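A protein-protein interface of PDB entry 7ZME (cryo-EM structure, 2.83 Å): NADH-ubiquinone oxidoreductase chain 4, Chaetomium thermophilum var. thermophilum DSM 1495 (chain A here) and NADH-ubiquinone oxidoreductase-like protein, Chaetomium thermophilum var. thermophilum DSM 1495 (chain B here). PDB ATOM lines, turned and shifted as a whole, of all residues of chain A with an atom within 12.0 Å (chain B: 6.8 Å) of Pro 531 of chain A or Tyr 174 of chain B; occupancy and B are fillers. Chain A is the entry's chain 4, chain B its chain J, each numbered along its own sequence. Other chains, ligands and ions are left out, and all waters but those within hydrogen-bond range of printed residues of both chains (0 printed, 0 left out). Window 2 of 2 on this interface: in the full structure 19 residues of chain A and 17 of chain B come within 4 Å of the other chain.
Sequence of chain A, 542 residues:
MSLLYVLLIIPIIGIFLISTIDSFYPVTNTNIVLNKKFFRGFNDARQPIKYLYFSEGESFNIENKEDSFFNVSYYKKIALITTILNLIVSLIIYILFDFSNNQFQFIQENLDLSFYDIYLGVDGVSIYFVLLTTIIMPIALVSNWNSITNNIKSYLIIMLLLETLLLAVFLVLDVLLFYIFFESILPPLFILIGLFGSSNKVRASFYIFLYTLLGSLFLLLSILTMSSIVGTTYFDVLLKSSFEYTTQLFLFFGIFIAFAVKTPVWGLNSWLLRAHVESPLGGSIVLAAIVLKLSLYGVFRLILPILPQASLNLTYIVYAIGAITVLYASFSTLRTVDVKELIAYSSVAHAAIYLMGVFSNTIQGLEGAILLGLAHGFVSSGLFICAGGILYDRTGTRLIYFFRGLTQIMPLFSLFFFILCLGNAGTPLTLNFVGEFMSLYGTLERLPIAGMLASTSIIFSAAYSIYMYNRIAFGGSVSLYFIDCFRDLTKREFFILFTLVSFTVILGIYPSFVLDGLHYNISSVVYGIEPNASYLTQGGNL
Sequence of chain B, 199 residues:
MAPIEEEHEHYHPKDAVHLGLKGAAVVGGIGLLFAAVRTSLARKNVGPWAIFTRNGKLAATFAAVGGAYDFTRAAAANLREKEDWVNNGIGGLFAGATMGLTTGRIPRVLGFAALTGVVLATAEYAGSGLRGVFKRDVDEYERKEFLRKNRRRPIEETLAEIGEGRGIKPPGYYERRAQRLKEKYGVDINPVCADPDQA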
ATOM      1  N   GLU A 445      28.413  20.057  -0.451  1.00  0.00           N
ATOM      2  CA  GLU A 445      27.369  19.075  -0.712  1.00  0.00           C
ATOM      3  C   GLU A 445      27.349  18.654  -2.178  1.00  0.00           C
ATOM      4  O   GLU A 445      26.891  17.553  -2.502  1.00  0.00           O
ATOM      5  CB  GLU A 445      26.020  19.645  -0.267  1.00  0.00           C
ATOM      6  CG  GLU A 445      24.797  18.860  -0.690  1.00  0.00           C
ATOM      7  CD  GLU A 445      23.513  19.476  -0.176  1.00  0.00           C
ATOM      8  OE1 GLU A 445      22.741  18.770   0.505  1.00  0.00           O
ATOM      9  OE2 GLU A 445      23.277  20.667  -0.441  1.00  0.00           O
ATOM     10  N   TYR A 527      18.305  22.395 -10.723  1.00  0.00           N
ATOM     11  CA  TYR A 527      18.112  21.337 -11.711  1.00  0.00           C
ATOM     12  C   TYR A 527      18.118  19.992 -10.997  1.00  0.00           C
ATOM     13  O   TYR A 527      19.169  19.531 -10.539  1.00  0.00           O
ATOM     14  CB  TYR A 527      19.197  21.394 -12.782  1.00  0.00           C
ATOM     15  CG  TYR A 527      18.938  20.511 -13.976  1.00  0.00           C
ATOM     16  CD1 TYR A 527      17.804  20.680 -14.756  1.00  0.00           C
ATOM     17  CD2 TYR A 527      19.831  19.507 -14.325  1.00  0.00           C
ATOM     18  CE1 TYR A 527      17.567  19.874 -15.849  1.00  0.00           C
ATOM     19  CE2 TYR A 527      19.605  18.700 -15.413  1.00  0.00           C
ATOM     20  CZ  TYR A 527      18.473  18.886 -16.173  1.00  0.00           C
ATOM     21  OH  TYR A 527      18.243  18.078 -17.260  1.00  0.00           O
ATOM     22  N   GLY A 528      16.958  19.365 -10.905  1.00  0.00           N
ATOM     23  CA  GLY A 528      16.855  18.072 -10.262  1.00  0.00           C
ATOM     24  C   GLY A 528      15.436  17.788  -9.835  1.00  0.00           C
ATOM     25  O   GLY A 528      14.569  18.659  -9.845  1.00  0.00           O
ATOM     26  N   ILE A 529      15.212  16.529  -9.463  1.00  0.00           N
ATOM     27  CA  ILE A 529      13.923  16.048  -8.980  1.00  0.00           C
ATOM     28  C   ILE A 529      14.162  15.017  -7.885  1.00  0.00           C
ATOM     29  O   ILE A 529      15.262  14.492  -7.719  1.00  0.00           O
ATOM     30  CB  ILE A 529      13.050  15.435 -10.101  1.00  0.00           C
ATOM     31  CG1 ILE A 529      13.741  14.218 -10.719  1.00  0.00           C
ATOM     32  CG2 ILE A 529      12.650  16.471 -11.141  1.00  0.00           C
ATOM     33  CD1 ILE A 529      12.853  13.432 -11.653  1.00  0.00           C
ATOM     34  N   GLU A 530      13.107  14.737  -7.134  1.00  0.00           N
ATOM     35  CA  GLU A 530      13.056  13.724  -6.099  1.00  0.00           C
ATOM     36  C   GLU A 530      12.337  12.482  -6.615  1.00  0.00           C
ATOM     37  O   GLU A 530      11.465  12.581  -7.482  1.00  0.00           O
ATOM     38  CB  GLU A 530      12.332  14.240  -4.849  1.00  0.00           C
ATOM     39  CG  GLU A 530      13.023  15.407  -4.159  1.00  0.00           C
ATOM     40  CD  GLU A 530      14.150  14.954  -3.254  1.00  0.00           C
ATOM     41  OE1 GLU A 530      14.144  13.776  -2.839  1.00  0.00           O
ATOM     42  OE2 GLU A 530      15.041  15.773  -2.955  1.00  0.00           O
ATOM     43  N   PRO A 531      12.694  11.295  -6.117  1.00  0.00           N
ATOM     44  CA  PRO A 531      12.038  10.070  -6.604  1.00  0.00           C
ATOM     45  C   PRO A 531      10.567   9.980  -6.245  1.00  0.00           C
ATOM     46  O   PRO A 531       9.842   9.214  -6.890  1.00  0.00           O
ATOM     47  CB  PRO A 531      12.839   8.950  -5.931  1.00  0.00           C
ATOM     48  CG  PRO A 531      14.104   9.590  -5.473  1.00  0.00           C
ATOM     49  CD  PRO A 531      13.755  10.994  -5.146  1.00  0.00           C
ATOM     50  N   ASN A 532      10.102  10.725  -5.243  1.00  0.00           N
ATOM     51  CA  ASN A 532       8.714  10.647  -4.807  1.00  0.00           C
ATOM     52  C   ASN A 532       8.056  12.016  -4.691  1.00  0.00           C
ATOM     53  O   ASN A 532       6.993  12.127  -4.071  1.00  0.00           O
ATOM     54  CB  ASN A 532       8.613   9.909  -3.468  1.00  0.00           C
ATOM     55  CG  ASN A 532       9.302   8.561  -3.494  1.00  0.00           C
ATOM     56  OD1 ASN A 532       8.928   7.676  -4.264  1.00  0.00           O
ATOM     57  ND2 ASN A 532      10.318   8.399  -2.656  1.00  0.00           N
ATOM     58  N   ALA A 533       8.656  13.059  -5.264  1.00  0.00           N
ATOM     59  CA  ALA A 533       8.090  14.401  -5.232  1.00  0.00           C
ATOM     60  C   ALA A 533       8.073  15.013  -6.625  1.00  0.00           C
ATOM     61  O   ALA A 533       8.124  16.236  -6.776  1.00  0.00           O
ATOM     62  CB  ALA A 533       8.854  15.300  -4.260  1.00  0.00           C
ATOM     63  N   SER A 534       8.003  14.170  -7.651  1.00  0.00           N
ATOM     64  CA  SER A 534       8.010  14.615  -9.034  1.00  0.00           C
ATOM     65  C   SER A 534       6.927  13.874  -9.799  1.00  0.00           C
ATOM     66  O   SER A 534       6.546  12.758  -9.440  1.00  0.00           O
ATOM     67  CB  SER A 534       9.369  14.374  -9.695  1.00  0.00           C
ATOM     68  OG  SER A 534       9.763  13.020  -9.553  1.00  0.00           O
ATOM     69  N   TYR A 535       6.435  14.515 -10.859  1.00  0.00           N
ATOM     70  CA  TYR A 535       5.442  13.919 -11.753  1.00  0.00           C
ATOM     71  C   TYR A 535       4.203  13.460 -10.987  1.00  0.00           C
ATOM     72  O   TYR A 535       3.640  12.399 -11.258  1.00  0.00           O
ATOM     73  CB  TYR A 535       6.050  12.765 -12.547  1.00  0.00           C
ATOM     74  CG  TYR A 535       7.261  13.167 -13.345  1.00  0.00           C
ATOM     75  CD1 TYR A 535       7.146  14.021 -14.429  1.00  0.00           C
ATOM     76  CD2 TYR A 535       8.521  12.708 -13.005  1.00  0.00           C
ATOM     77  CE1 TYR A 535       8.252  14.396 -15.158  1.00  0.00           C
ATOM     78  CE2 TYR A 535       9.631  13.080 -13.727  1.00  0.00           C
ATOM     79  CZ  TYR A 535       9.492  13.923 -14.803  1.00  0.00           C
ATOM     80  OH  TYR A 535      10.597  14.295 -15.526  1.00  0.00           O
ATOM     81  N   LEU A 536       3.777  14.268 -10.022  1.00  0.00           N
ATOM     82  CA  LEU A 536       2.615  13.922  -9.218  1.00  0.00           C
ATOM     83  C   LEU A 536       1.341  14.038 -10.045  1.00  0.00           C
ATOM     84  O   LEU A 536       1.217  14.912 -10.908  1.00  0.00           O
ATOM     85  CB  LEU A 536       2.532  14.826  -7.989  1.00  0.00           C
ATOM     86  CG  LEU A 536       3.849  15.112  -7.264  1.00  0.00           C
ATOM     87  CD1 LEU A 536       3.613  16.016  -6.062  1.00  0.00           C
ATOM     88  CD2 LEU A 536       4.528  13.821  -6.837  1.00  0.00           C
ATOM     89  N   THR A 537       0.393  13.146  -9.781  1.00  0.00           N
ATOM     90  CA  THR A 537      -0.879  13.148 -10.494  1.00  0.00           C
ATOM     91  C   THR A 537      -2.050  13.189  -9.521  1.00  0.00           C
ATOM     92  O   THR A 537      -2.697  14.224  -9.355  1.00  0.00           O
ATOM     93  CB  THR A 537      -1.018  11.913 -11.403  1.00  0.00           C
ATOM     94  OG1 THR A 537      -0.759  10.724 -10.644  1.00  0.00           O
ATOM     95  CG2 THR A 537      -0.041  11.990 -12.564  1.00  0.00           C
ATOM     96  N   GLU B 164      22.532   9.359 -13.461  1.00  0.00           N
ATOM     97  CA  GLU B 164      21.507   9.346 -12.430  1.00  0.00           C
ATOM     98  C   GLU B 164      22.168   9.617 -11.088  1.00  0.00           C
ATOM     99  O   GLU B 164      23.147   8.953 -10.729  1.00  0.00           O
ATOM    100  CB  GLU B 164      20.774   8.007 -12.414  1.00  0.00           C
ATOM    101  CG  GLU B 164      19.626   7.945 -11.447  1.00  0.00           C
ATOM    102  CD  GLU B 164      18.862   6.642 -11.541  1.00  0.00           C
ATOM    103  OE1 GLU B 164      19.281   5.760 -12.319  1.00  0.00           O
ATOM    104  OE2 GLU B 164      17.835   6.503 -10.846  1.00  0.00           O
ATOM    105  N   LYS B 169      17.288  12.402  -9.305  1.00  0.00           N
ATOM    106  CA  LYS B 169      16.748  11.276  -8.548  1.00  0.00           C
ATOM    107  C   LYS B 169      15.369  10.977  -9.115  1.00  0.00           C
ATOM    108  O   LYS B 169      14.348  11.382  -8.545  1.00  0.00           O
ATOM    109  CB  LYS B 169      16.688  11.608  -7.058  1.00  0.00           C
ATOM    110  CG  LYS B 169      18.020  11.522  -6.326  1.00  0.00           C
ATOM    111  CD  LYS B 169      17.814  11.262  -4.844  1.00  0.00           C
ATOM    112  CE  LYS B 169      19.132  11.031  -4.121  1.00  0.00           C
ATOM    113  NZ  LYS B 169      19.109   9.818  -3.260  1.00  0.00           N
ATOM    114  N   PRO B 170      15.302  10.285 -10.247  1.00  0.00           N
ATOM    115  CA  PRO B 170      14.013  10.021 -10.888  1.00  0.00           C
ATOM    116  C   PRO B 170      13.213   9.021 -10.075  1.00  0.00           C
ATOM    117  O   PRO B 170      13.772   8.350  -9.196  1.00  0.00           O
ATOM    118  CB  PRO B 170      14.416   9.441 -12.256  1.00  0.00           C
ATOM    119  CG  PRO B 170      15.892   9.673 -12.376  1.00  0.00           C
ATOM    120  CD  PRO B 170      16.414   9.680 -10.992  1.00  0.00           C
ATOM    121  N   PRO B 171      11.908   8.894 -10.314  1.00  0.00           N
ATOM    122  CA  PRO B 171      11.137   7.907  -9.551  1.00  0.00           C
ATOM    123  C   PRO B 171      11.669   6.502  -9.779  1.00  0.00           C
ATOM    124  O   PRO B 171      12.011   6.118 -10.898  1.00  0.00           O
ATOM    125  CB  PRO B 171       9.704   8.078 -10.079  1.00  0.00           C
ATOM    126  CG  PRO B 171       9.748   9.229 -11.046  1.00  0.00           C
ATOM    127  CD  PRO B 171      11.152   9.393 -11.473  1.00  0.00           C
ATOM    128  N   GLY B 172      11.740   5.736  -8.694  1.00  0.00           N
ATOM    129  CA  GLY B 172      12.403   4.450  -8.716  1.00  0.00           C
ATOM    130  C   GLY B 172      13.897   4.501  -8.499  1.00  0.00           C
ATOM    131  O   GLY B 172      14.566   3.476  -8.663  1.00  0.00           O
ATOM    132  N   TYR B 173      14.443   5.666  -8.140  1.00  0.00           N
ATOM    133  CA  TYR B 173      15.881   5.787  -7.914  1.00  0.00           C
ATOM    134  C   TYR B 173      16.329   4.945  -6.729  1.00  0.00           C
ATOM    135  O   TYR B 173      17.367   4.277  -6.789  1.00  0.00           O
ATOM    136  CB  TYR B 173      16.251   7.255  -7.691  1.00  0.00           C
ATOM    137  CG  TYR B 173      17.677   7.476  -7.235  1.00  0.00           C
ATOM    138  CD1 TYR B 173      18.699   7.640  -8.154  1.00  0.00           C
ATOM    139  CD2 TYR B 173      18.000   7.518  -5.888  1.00  0.00           C
ATOM    140  CE1 TYR B 173      19.993   7.835  -7.752  1.00  0.00           C
ATOM    141  CE2 TYR B 173      19.293   7.706  -5.479  1.00  0.00           C
ATOM    142  CZ  TYR B 173      20.287   7.870  -6.414  1.00  0.00           C
ATOM    143  OH  TYR B 173      21.586   8.068  -6.003  1.00  0.00           O
ATOM    144  N   TYR B 174      15.567   4.973  -5.636  1.00  0.00           N
ATOM    145  CA  TYR B 174      16.008   4.332  -4.403  1.00  0.00           C
ATOM    146  C   TYR B 174      16.056   2.817  -4.546  1.00  0.00           C
ATOM    147  O   TYR B 174      16.977   2.170  -4.033  1.00  0.00           O
ATOM    148  CB  TYR B 174      15.093   4.740  -3.251  1.00  0.00           C
ATOM    149  CG  TYR B 174      15.428   6.091  -2.661  1.00  0.00           C
ATOM    150  CD1 TYR B 174      16.696   6.356  -2.163  1.00  0.00           C
ATOM    151  CD2 TYR B 174      14.477   7.099  -2.605  1.00  0.00           C
ATOM    152  CE1 TYR B 174      17.008   7.591  -1.623  1.00  0.00           C
ATOM    153  CE2 TYR B 174      14.778   8.335  -2.068  1.00  0.00           C
ATOM    154  CZ  TYR B 174      16.045   8.576  -1.578  1.00  0.00           C
ATOM    155  OH  TYR B 174      16.347   9.807  -1.042  1.00  0.00           O
ATOM    156  N   GLU B 175      15.068   2.233  -5.225  1.00  0.00           N
ATOM    157  CA  GLU B 175      15.092   0.794  -5.468  1.00  0.00           C
ATOM    158  C   GLU B 175      16.276   0.406  -6.342  1.00  0.00           C
ATOM    159  O   GLU B 175      16.912  -0.630  -6.115  1.00  0.00           O
ATOM    160  CB  GLU B 175      13.778   0.349  -6.109  1.00  0.00           C
ATOM    161  N   ARG B 176      16.583   1.222  -7.352  1.00  0.00           N
ATOM    162  CA  ARG B 176      17.747   0.956  -8.190  1.00  0.00           C
ATOM    163  C   ARG B 176      19.033   1.059  -7.386  1.00  0.00           C
ATOM    164  O   ARG B 176      19.971   0.281  -7.595  1.00  0.00           O
ATOM    165  CB  ARG B 176      17.780   1.928  -9.368  1.00  0.00           C
ATOM    166  CG  ARG B 176      17.190   1.382 -10.649  1.00  0.00           C
ATOM    167  CD  ARG B 176      17.049   2.485 -11.676  1.00  0.00           C
ATOM    168  NE  ARG B 176      16.293   3.615 -11.149  1.00  0.00           N
ATOM    169  CZ  ARG B 176      15.663   4.505 -11.905  1.00  0.00           C
ATOM    170  NH1 ARG B 176      14.997   5.503 -11.341  1.00  0.00           N
ATOM    171  NH2 ARG B 176      15.699   4.399 -13.225  1.00  0.00           N
ATOM    172  N   ARG B 177      19.096   2.025  -6.468  1.00  0.00           N
ATOM    173  CA  ARG B 177      20.273   2.175  -5.621  1.00  0.00           C
ATOM    174  C   ARG B 177      20.487   0.951  -4.744  1.00  0.00           C
ATOM    175  O   ARG B 177      21.627   0.519  -4.538  1.00  0.00           O
ATOM    176  CB  ARG B 177      20.135   3.428  -4.760  1.00  0.00           C
ATOM    177  CG  ARG B 177      21.325   3.682  -3.868  1.00  0.00           C
ATOM    178  CD  ARG B 177      21.196   4.990  -3.124  1.00  0.00           C
ATOM    179  NE  ARG B 177      22.305   5.176  -2.196  1.00  0.00           N
ATOM    180  CZ  ARG B 177      22.285   4.790  -0.925  1.00  0.00           C
ATOM    181  NH1 ARG B 177      23.342   4.994  -0.150  1.00  0.00           N
ATOM    182  NH2 ARG B 177      21.209   4.196  -0.429  1.00  0.00           N
ATOM    183  N   ALA B 178      19.403   0.381  -4.214  1.00  0.00           N
ATOM    184  CA  ALA B 178      19.532  -0.785  -3.347  1.00  0.00           C
ATOM    185  C   ALA B 178      20.136  -1.965  -4.094  1.00  0.00           C
ATOM    186  O   ALA B 178      21.004  -2.668  -3.565  1.00  0.00           O
ATOM    187  CB  ALA B 178      18.171  -1.157  -2.763  1.00  0.00           C
ATOM    188  N   GLN B 179      19.685  -2.201  -5.327  1.00  0.00           N
ATOM    189  CA  GLN B 179      20.246  -3.288  -6.121  1.00  0.00           C
ATOM    190  C   GLN B 179      21.688  -2.998  -6.518  1.00  0.00           C
ATOM    191  O   GLN B 179      22.543  -3.890  -6.464  1.00  0.00           O
ATOM    192  CB  GLN B 179      19.386  -3.531  -7.360  1.00  0.00           C
ATOM    193  CG  GLN B 179      17.980  -4.016  -7.052  1.00  0.00           C
ATOM    194  CD  GLN B 179      17.200  -4.370  -8.304  1.00  0.00           C
ATOM    195  OE1 GLN B 179      17.779  -4.723  -9.331  1.00  0.00           O
ATOM    196  NE2 GLN B 179      15.877  -4.276  -8.222  1.00  0.00           N
ATOM    197  N   ILE B 189      20.166  -3.248   2.199  1.00  0.00           N
ATOM    198  CA  ILE B 189      19.857  -1.907   2.682  1.00  0.00           C
ATOM    199  C   ILE B 189      18.568  -1.958   3.495  1.00  0.00           C
ATOM    200  O   ILE B 189      17.526  -2.396   2.999  1.00  0.00           O
ATOM    201  CB  ILE B 189      19.738  -0.914   1.519  1.00  0.00           C
ATOM    202  CG1 ILE B 189      21.120  -0.632   0.922  1.00  0.00           C
ATOM    203  CG2 ILE B 189      19.071   0.373   1.977  1.00  0.00           C
ATOM    204  CD1 ILE B 189      21.931   0.379   1.698  1.00  0.00           C
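Printed residues of chain A that touch a printed residue of chain B: Ile 529, Glu 530 and Pro 531.
Along chain A the printed residues that touch a printed residue of chain B span positions 529 to 531.
O of Glu 530 of chain A lies close to O of Lys 169 of chain B, 3.3 Å away.
The backbone NH of Lys 169 of chain B lies close to the backbone carbonyl oxygen of Ile 529 of chain A, 3.3 Å away.
The backbone carbonyl oxygen (O) of Lys 169 of chain B sits close to the backbone nitrogen (N) of Pro 531 of chain A (2.9 Å).
The backbone carbonyl oxygen (O) of Pro 171 of chain B sits at hydrogen-bond distance from the guanidinium group (NH1) of Arg 176 of chain B.
The backbone carbonyl oxygen (O) of Glu 530 of chain A is in hydrogen-bond range of the side-chain hydroxyl (OG) of Ser 534 of chain A, 2.7 Å away.
Of chain B, only Lys 169, Pro 170, Pro 171, Tyr 173 and Tyr 174 come within 4 Å of Pro 531 of chain A.
Tyr 174 of chain B touches just one residue of chain A: Pro 531 (3.7 Å).
Of chain A, only Pro 531 comes within 4 Å of Pro 171 of chain B.
Tyr 173 of chain B touches one residue of chain A.
No residue of chain A comes within 4 Å of Glu 175 of chain B.
No residue of chain A comes within 4 Å of Arg 176 of chain B.
Arg 177 of chain B touches none of the printed residues of chain A.
No residue of chain A comes within 4 Å of Ala 178 of chain B.
Of the printed residues of chain B, Ile 529 of chain A touches Lys 169 (3.3 Å) and Pro 170 (3.7 Å).
Of the printed residues of chain B, Glu 530 of chain A touches Lys 169 (3.0 Å).
Glu 445 of chain A touches none of the printed residues of chain B.
The nearest residue of chain A that does not touch Tyr 174 of chain B is Asn 532 of chain A (4.4 Å).
Among the printed residues, pairs that only touch across the chains: Pro 531 of chain A with Pro 171 of chain B, Pro 531 of chain A with Pro 170 of chain B, Ile 529 of chain A with Pro 170 of chain B, Pro 531 of chain A with Tyr 174 of chain B and Pro 531 of chain A with Tyr 173 of chain B.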
